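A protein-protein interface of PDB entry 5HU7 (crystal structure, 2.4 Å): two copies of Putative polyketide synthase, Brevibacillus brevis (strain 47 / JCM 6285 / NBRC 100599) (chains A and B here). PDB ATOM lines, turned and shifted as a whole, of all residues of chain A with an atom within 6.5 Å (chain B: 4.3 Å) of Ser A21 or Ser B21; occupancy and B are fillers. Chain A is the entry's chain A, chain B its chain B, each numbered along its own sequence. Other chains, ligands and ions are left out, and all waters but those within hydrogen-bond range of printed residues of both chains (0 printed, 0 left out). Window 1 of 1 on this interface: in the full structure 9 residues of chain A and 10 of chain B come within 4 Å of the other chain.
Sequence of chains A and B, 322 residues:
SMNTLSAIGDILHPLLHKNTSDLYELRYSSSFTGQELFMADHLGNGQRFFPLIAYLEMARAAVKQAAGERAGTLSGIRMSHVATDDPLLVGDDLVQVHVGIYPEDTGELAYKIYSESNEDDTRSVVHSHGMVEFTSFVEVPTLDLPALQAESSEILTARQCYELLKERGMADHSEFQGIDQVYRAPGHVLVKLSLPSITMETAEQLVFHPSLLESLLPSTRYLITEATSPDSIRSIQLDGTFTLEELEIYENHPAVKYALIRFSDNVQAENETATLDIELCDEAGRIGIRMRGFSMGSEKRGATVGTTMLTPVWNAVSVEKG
The side-chain amide nitrogen (ND2) of Asn A19 is in hydrogen-bond range of the backbone carbonyl oxygen (O) of Ser B21, 2.9 Å away. ND2 of Asn B19 is in hydrogen-bond range of O of Ser A21, 3.0 Å away.
OD1 of Asn A19 lies within hydrogen-bond range of OG of Ser A21 (2.7 Å). OD1 of Asn A19 lies close to O of Arg A27, 3.3 Å away. OH of Tyr A28 lies within hydrogen-bond range of N of Ala A66, 3.2 Å away. The side-chain hydroxyl of Ser B21 lies within hydrogen-bond range of the side-chain amide oxygen of Asn B19 (2.7 Å). The backbone carbonyl oxygen (O) of Arg B27 sits close to the side-chain amide oxygen (OD1) of Asn B19 (3.3 Å). N of Glu B25 is in hydrogen-bond range of OD1 of Asp B22 (2.9 Å).
Asn A19 touches Asn B19. C of Thr B20 touches ND2 of Asn A19 (3.97 Å). CB of Ser B21 touches CB of Ser A21 (3.7 Å). Leu A26 touches Ser B21. Leu A26 touches Asp B22 (CD1 to O, 3.7 Å). Tyr A28 touches Ser B21 (OH to O, 3.96 Å).
Of chain B, only Asn B19 and Ser B21 come within 4 Å of Ser A21. Ser B21 touches just these residues of chain A: Asn A19 (2.9 Å), Ser A21 (3.7 Å), Leu A26 (3.9 Å) and Tyr A28 (3.96 Å). Of the printed residues of chain A, Thr B20 touches Asn A19 (3.97 Å). Printed residues of chain A within 4 Å of Asn B19: Asn A19 (3.4 Å) and Ser A21 (3.0 Å). The nearest printed residue of chain A that does not touch Asn B19 is Thr A20 (4.2 Å).
Of the 7 printed residues of chain B, 4 touch a printed residue of chain A. Among the printed residues, 8 pairs touch across the chains.
Asn B19 touches its own counterpart, Asn A19. Asn A19 touches Thr B20, but with the chains exchanged Thr A20 does not touch Asn B19 (4.2 Å). Ser B21 touches its own counterpart, Ser A21. Leu A26 touches Asp B22, but with the chains exchanged Asp A22 does not touch Leu B26 (4.04 Å). Positions printed for both chains: 19, 20, 21, 22, 25, 26 and 27. Of the 8 pairs that touch across the chains among the printed residues, 4 have their exchanged pair printed and touching as well.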
ATOM      1  N   LYS A  18       1.264 -23.168 -30.548  1.00  0.00           N
ATOM      2  CA  LYS A  18       0.869 -22.021 -29.732  1.00  0.00           C
ATOM      3  C   LYS A  18      -0.550 -21.613 -29.913  1.00  0.00           C
ATOM      4  O   LYS A  18      -1.095 -21.727 -30.998  1.00  0.00           O
ATOM      5  CB  LYS A  18       1.732 -20.773 -30.084  1.00  0.00           C
ATOM      6  CG  LYS A  18       3.154 -20.774 -29.552  1.00  0.00           C
ATOM      7  CD  LYS A  18       3.197 -20.732 -28.012  1.00  0.00           C
ATOM      8  CE  LYS A  18       4.547 -20.354 -27.442  1.00  0.00           C
ATOM      9  NZ  LYS A  18       5.589 -21.372 -27.728  1.00  0.00           N
ATOM     10  N   ASN A  19      -1.085 -20.962 -28.885  1.00  0.00           N
ATOM     11  CA  ASN A  19      -2.407 -20.385 -28.913  1.00  0.00           C
ATOM     12  C   ASN A  19      -2.158 -18.960 -29.364  1.00  0.00           C
ATOM     13  O   ASN A  19      -1.467 -18.234 -28.667  1.00  0.00           O
ATOM     14  CB  ASN A  19      -3.037 -20.420 -27.538  1.00  0.00           C
ATOM     15  CG  ASN A  19      -4.436 -19.881 -27.520  1.00  0.00           C
ATOM     16  OD1 ASN A  19      -4.792 -19.020 -28.312  1.00  0.00           O
ATOM     17  ND2 ASN A  19      -5.259 -20.372 -26.633  1.00  0.00           N
ATOM     18  N   THR A  20      -2.681 -18.569 -30.532  1.00  0.00           N
ATOM     19  CA  THR A  20      -2.486 -17.220 -31.057  1.00  0.00           C
ATOM     20  C   THR A  20      -3.826 -16.497 -31.200  1.00  0.00           C
ATOM     21  O   THR A  20      -3.982 -15.644 -32.077  1.00  0.00           O
ATOM     22  CB  THR A  20      -1.742 -17.268 -32.393  1.00  0.00           C
ATOM     23  OG1 THR A  20      -2.556 -17.968 -33.342  1.00  0.00           O
ATOM     24  CG2 THR A  20      -0.390 -17.864 -32.266  1.00  0.00           C
ATOM     25  N   SER A  21      -4.773 -16.803 -30.317  1.00  0.00           N
ATOM     26  CA  SER A  21      -6.081 -16.172 -30.342  1.00  0.00           C
ATOM     27  C   SER A  21      -5.965 -14.683 -30.136  1.00  0.00           C
ATOM     28  O   SER A  21      -5.091 -14.241 -29.407  1.00  0.00           O
ATOM     29  CB  SER A  21      -6.959 -16.738 -29.239  1.00  0.00           C
ATOM     30  OG  SER A  21      -7.064 -18.137 -29.427  1.00  0.00           O
ATOM     31  N   ASP A  22      -6.844 -13.918 -30.758  1.00  0.00           N
ATOM     32  CA  ASP A  22      -6.825 -12.459 -30.657  1.00  0.00           C
ATOM     33  C   ASP A  22      -8.242 -11.942 -30.637  1.00  0.00           C
ATOM     34  O   ASP A  22      -9.168 -12.751 -30.479  1.00  0.00           O
ATOM     35  CB  ASP A  22      -5.960 -11.858 -31.802  1.00  0.00           C
ATOM     36  CG  ASP A  22      -6.476 -11.968 -33.227  1.00  0.00           C
ATOM     37  OD1 ASP A  22      -7.544 -12.584 -33.436  1.00  0.00           O
ATOM     38  OD2 ASP A  22      -5.792 -11.470 -34.136  1.00  0.00           O
ATOM     39  N   LEU A  23      -8.430 -10.608 -30.751  1.00  0.00           N
ATOM     40  CA  LEU A  23      -9.763  -9.989 -30.767  1.00  0.00           C
ATOM     41  C   LEU A  23     -10.670 -10.542 -31.839  1.00  0.00           C
ATOM     42  O   LEU A  23     -11.867 -10.664 -31.615  1.00  0.00           O
ATOM     43  CB  LEU A  23      -9.655  -8.477 -31.007  1.00  0.00           C
ATOM     44  CG  LEU A  23      -9.325  -7.654 -29.796  1.00  0.00           C
ATOM     45  CD1 LEU A  23      -8.869  -6.270 -30.204  1.00  0.00           C
ATOM     46  CD2 LEU A  23     -10.518  -7.577 -28.850  1.00  0.00           C
ATOM     47  N   TYR A  24     -10.107 -10.836 -32.998  1.00  0.00           N
ATOM     48  CA  TYR A  24     -10.857 -11.276 -34.158  1.00  0.00           C
ATOM     49  C   TYR A  24     -11.020 -12.766 -34.303  1.00  0.00           C
ATOM     50  O   TYR A  24     -11.823 -13.156 -35.138  1.00  0.00           O
ATOM     51  CB  TYR A  24     -10.205 -10.700 -35.422  1.00  0.00           C
ATOM     52  CG  TYR A  24      -9.972  -9.209 -35.282  1.00  0.00           C
ATOM     53  CD1 TYR A  24     -11.043  -8.328 -35.154  1.00  0.00           C
ATOM     54  CD2 TYR A  24      -8.694  -8.699 -35.087  1.00  0.00           C
ATOM     55  CE1 TYR A  24     -10.843  -6.965 -34.943  1.00  0.00           C
ATOM     56  CE2 TYR A  24      -8.478  -7.339 -34.875  1.00  0.00           C
ATOM     57  CZ  TYR A  24      -9.556  -6.470 -34.812  1.00  0.00           C
ATOM     58  OH  TYR A  24      -9.372  -5.118 -34.602  1.00  0.00           O
ATOM     59  N   GLU A  25     -10.295 -13.615 -33.526  1.00  0.00           N
ATOM     60  CA  GLU A  25     -10.382 -15.072 -33.711  1.00  0.00           C
ATOM     61  C   GLU A  25      -9.786 -15.911 -32.583  1.00  0.00           C
ATOM     62  O   GLU A  25      -8.748 -15.532 -32.058  1.00  0.00           O
ATOM     63  CB  GLU A  25      -9.605 -15.386 -34.996  1.00  0.00           C
ATOM     64  CG  GLU A  25      -9.828 -16.752 -35.635  1.00  0.00           C
ATOM     65  CD  GLU A  25      -9.016 -16.924 -36.912  1.00  0.00           C
ATOM     66  OE1 GLU A  25      -8.208 -16.029 -37.239  1.00  0.00           O
ATOM     67  OE2 GLU A  25      -9.187 -17.955 -37.594  1.00  0.00           O
ATOM     68  N   LEU A  26     -10.387 -17.092 -32.283  1.00  0.00           N
ATOM     69  CA  LEU A  26      -9.866 -18.119 -31.354  1.00  0.00           C
ATOM     70  C   LEU A  26      -9.067 -19.068 -32.257  1.00  0.00           C
ATOM     71  O   LEU A  26      -9.667 -19.706 -33.130  1.00  0.00           O
ATOM     72  CB  LEU A  26     -11.002 -18.919 -30.655  1.00  0.00           C
ATOM     73  CG  LEU A  26     -10.619 -20.165 -29.828  1.00  0.00           C
ATOM     74  CD1 LEU A  26      -9.824 -19.828 -28.614  1.00  0.00           C
ATOM     75  CD2 LEU A  26     -11.844 -20.880 -29.331  1.00  0.00           C
ATOM     76  N   ARG A  27      -7.723 -19.122 -32.101  1.00  0.00           N
ATOM     77  CA  ARG A  27      -6.918 -19.968 -32.981  1.00  0.00           C
ATOM     78  C   ARG A  27      -5.595 -20.420 -32.420  1.00  0.00           C
ATOM     79  O   ARG A  27      -5.090 -19.892 -31.452  1.00  0.00           O
ATOM     80  CB  ARG A  27      -6.678 -19.292 -34.340  1.00  0.00           C
ATOM     81  CG  ARG A  27      -5.720 -18.130 -34.293  1.00  0.00           C
ATOM     82  CD  ARG A  27      -5.342 -17.645 -35.676  1.00  0.00           C
ATOM     83  NE  ARG A  27      -4.333 -16.585 -35.626  1.00  0.00           N
ATOM     84  CZ  ARG A  27      -3.905 -15.893 -36.685  1.00  0.00           C
ATOM     85  NH1 ARG A  27      -4.399 -16.135 -37.901  1.00  0.00           N
ATOM     86  NH2 ARG A  27      -2.980 -14.947 -36.534  1.00  0.00           N
ATOM     87  N   TYR A  28      -5.039 -21.435 -33.069  1.00  0.00           N
ATOM     88  CA  TYR A  28      -3.756 -22.016 -32.719  1.00  0.00           C
ATOM     89  C   TYR A  28      -2.870 -21.976 -33.961  1.00  0.00           C
ATOM     90  O   TYR A  28      -3.380 -22.005 -35.079  1.00  0.00           O
ATOM     91  CB  TYR A  28      -3.955 -23.439 -32.178  1.00  0.00           C
ATOM     92  CG  TYR A  28      -4.951 -23.497 -31.042  1.00  0.00           C
ATOM     93  CD1 TYR A  28      -6.315 -23.563 -31.287  1.00  0.00           C
ATOM     94  CD2 TYR A  28      -4.536 -23.338 -29.721  1.00  0.00           C
ATOM     95  CE1 TYR A  28      -7.247 -23.486 -30.250  1.00  0.00           C
ATOM     96  CE2 TYR A  28      -5.456 -23.329 -28.671  1.00  0.00           C
ATOM     97  CZ  TYR A  28      -6.813 -23.428 -28.940  1.00  0.00           C
ATOM     98  OH  TYR A  28      -7.755 -23.362 -27.944  1.00  0.00           O
ATOM     99  N   GLN A  65      -8.184 -28.226 -26.599  1.00  0.00           N
ATOM    100  CA  GLN A  65      -7.593 -27.019 -25.974  1.00  0.00           C
ATOM    101  C   GLN A  65      -8.662 -25.952 -25.750  1.00  0.00           C
ATOM    102  O   GLN A  65      -8.713 -25.375 -24.689  1.00  0.00           O
ATOM    103  CB  GLN A  65      -6.457 -26.419 -26.838  1.00  0.00           C
ATOM    104  CG  GLN A  65      -5.168 -27.204 -26.783  1.00  0.00           C
ATOM    105  CD  GLN A  65      -4.490 -27.130 -25.446  1.00  0.00           C
ATOM    106  OE1 GLN A  65      -4.403 -26.070 -24.825  1.00  0.00           O
ATOM    107  NE2 GLN A  65      -3.943 -28.246 -24.984  1.00  0.00           N
ATOM    108  N   ALA A  66      -9.508 -25.712 -26.753  1.00  0.00           N
ATOM    109  CA  ALA A  66     -10.656 -24.806 -26.699  1.00  0.00           C
ATOM    110  C   ALA A  66     -11.855 -25.462 -25.919  1.00  0.00           C
ATOM    111  O   ALA A  66     -12.837 -25.856 -26.539  1.00  0.00           O
ATOM    112  CB  ALA A  66     -11.087 -24.485 -28.130  1.00  0.00           C
ATOM    113  N   ASN B  19      -0.783 -17.277 -23.667  1.00  0.00           N
ATOM    114  CA  ASN B  19      -2.133 -16.985 -24.117  1.00  0.00           C
ATOM    115  C   ASN B  19      -2.875 -18.262 -23.830  1.00  0.00           C
ATOM    116  O   ASN B  19      -2.516 -19.296 -24.390  1.00  0.00           O
ATOM    117  CB  ASN B  19      -2.151 -16.670 -25.611  1.00  0.00           C
ATOM    118  CG  ASN B  19      -3.508 -16.308 -26.112  1.00  0.00           C
ATOM    119  OD1 ASN B  19      -4.520 -16.761 -25.589  1.00  0.00           O
ATOM    120  ND2 ASN B  19      -3.572 -15.485 -27.124  1.00  0.00           N
ATOM    121  N   THR B  20      -3.873 -18.220 -22.944  1.00  0.00           N
ATOM    122  CA  THR B  20      -4.653 -19.409 -22.593  1.00  0.00           C
ATOM    123  C   THR B  20      -6.139 -19.205 -22.947  1.00  0.00           C
ATOM    124  O   THR B  20      -7.021 -19.763 -22.294  1.00  0.00           O
ATOM    125  CB  THR B  20      -4.477 -19.737 -21.114  1.00  0.00           C
ATOM    126  OG1 THR B  20      -4.994 -18.658 -20.344  1.00  0.00           O
ATOM    127  CG2 THR B  20      -3.070 -20.038 -20.759  1.00  0.00           C
ATOM    128  N   SER B  21      -6.405 -18.452 -24.007  1.00  0.00           N
ATOM    129  CA  SER B  21      -7.769 -18.205 -24.452  1.00  0.00           C
ATOM    130  C   SER B  21      -8.465 -19.490 -24.826  1.00  0.00           C
ATOM    131  O   SER B  21      -7.828 -20.405 -25.315  1.00  0.00           O
ATOM    132  CB  SER B  21      -7.759 -17.287 -25.660  1.00  0.00           C
ATOM    133  OG  SER B  21      -7.111 -16.086 -25.317  1.00  0.00           O
ATOM    134  N   ASP B  22      -9.762 -19.555 -24.608  1.00  0.00           N
ATOM    135  CA  ASP B  22     -10.565 -20.735 -24.926  1.00  0.00           C
ATOM    136  C   ASP B  22     -11.920 -20.294 -25.451  1.00  0.00           C
ATOM    137  O   ASP B  22     -12.090 -19.101 -25.736  1.00  0.00           O
ATOM    138  CB  ASP B  22     -10.644 -21.664 -23.694  1.00  0.00           C
ATOM    139  CG  ASP B  22     -11.446 -21.193 -22.487  1.00  0.00           C
ATOM    140  OD1 ASP B  22     -11.954 -20.056 -22.514  1.00  0.00           O
ATOM    141  OD2 ASP B  22     -11.529 -21.950 -21.505  1.00  0.00           O
ATOM    142  N   GLU B  25     -13.449 -17.594 -23.069  1.00  0.00           N
ATOM    143  CA  GLU B  25     -12.737 -16.371 -22.675  1.00  0.00           C
ATOM    144  C   GLU B  25     -11.435 -16.115 -23.440  1.00  0.00           C
ATOM    145  O   GLU B  25     -10.699 -17.047 -23.700  1.00  0.00           O
ATOM    146  CB  GLU B  25     -12.380 -16.536 -21.189  1.00  0.00           C
ATOM    147  CG  GLU B  25     -11.973 -15.291 -20.434  1.00  0.00           C
ATOM    148  CD  GLU B  25     -11.668 -15.592 -18.979  1.00  0.00           C
ATOM    149  OE1 GLU B  25     -11.667 -16.781 -18.586  1.00  0.00           O
ATOM    150  OE2 GLU B  25     -11.439 -14.629 -18.219  1.00  0.00           O
ATOM    151  N   LEU B  26     -11.128 -14.835 -23.721  1.00  0.00           N
ATOM    152  CA  LEU B  26      -9.852 -14.357 -24.302  1.00  0.00           C
ATOM    153  C   LEU B  26      -8.996 -14.016 -23.080  1.00  0.00           C
ATOM    154  O   LEU B  26      -9.363 -13.113 -22.335  1.00  0.00           O
ATOM    155  CB  LEU B  26     -10.046 -13.095 -25.184  1.00  0.00           C
ATOM    156  CG  LEU B  26      -8.792 -12.342 -25.670  1.00  0.00           C
ATOM    157  CD1 LEU B  26      -7.985 -13.146 -26.635  1.00  0.00           C
ATOM    158  CD2 LEU B  26      -9.171 -11.069 -26.383  1.00  0.00           C
ATOM    159  N   ARG B  27      -7.903 -14.761 -22.828  1.00  0.00           N
ATOM    160  CA  ARG B  27      -7.103 -14.510 -21.636  1.00  0.00           C
ATOM    161  C   ARG B  27      -5.661 -14.934 -21.724  1.00  0.00           C
ATOM    162  O   ARG B  27      -5.272 -15.707 -22.581  1.00  0.00           O
ATOM    163  CB  ARG B  27      -7.738 -15.146 -20.381  1.00  0.00           C
ATOM    164  CG  ARG B  27      -7.644 -16.645 -20.327  1.00  0.00           C
ATOM    165  CD  ARG B  27      -8.076 -17.208 -18.991  1.00  0.00           C
ATOM    166  NE  ARG B  27      -7.892 -18.662 -18.918  1.00  0.00           N
ATOM    167  CZ  ARG B  27      -8.287 -19.434 -17.905  1.00  0.00           C
ATOM    168  NH1 ARG B  27      -8.907 -18.908 -16.857  1.00  0.00           N
ATOM    169  NH2 ARG B  27      -8.067 -20.746 -17.939  1.00  0.00           N
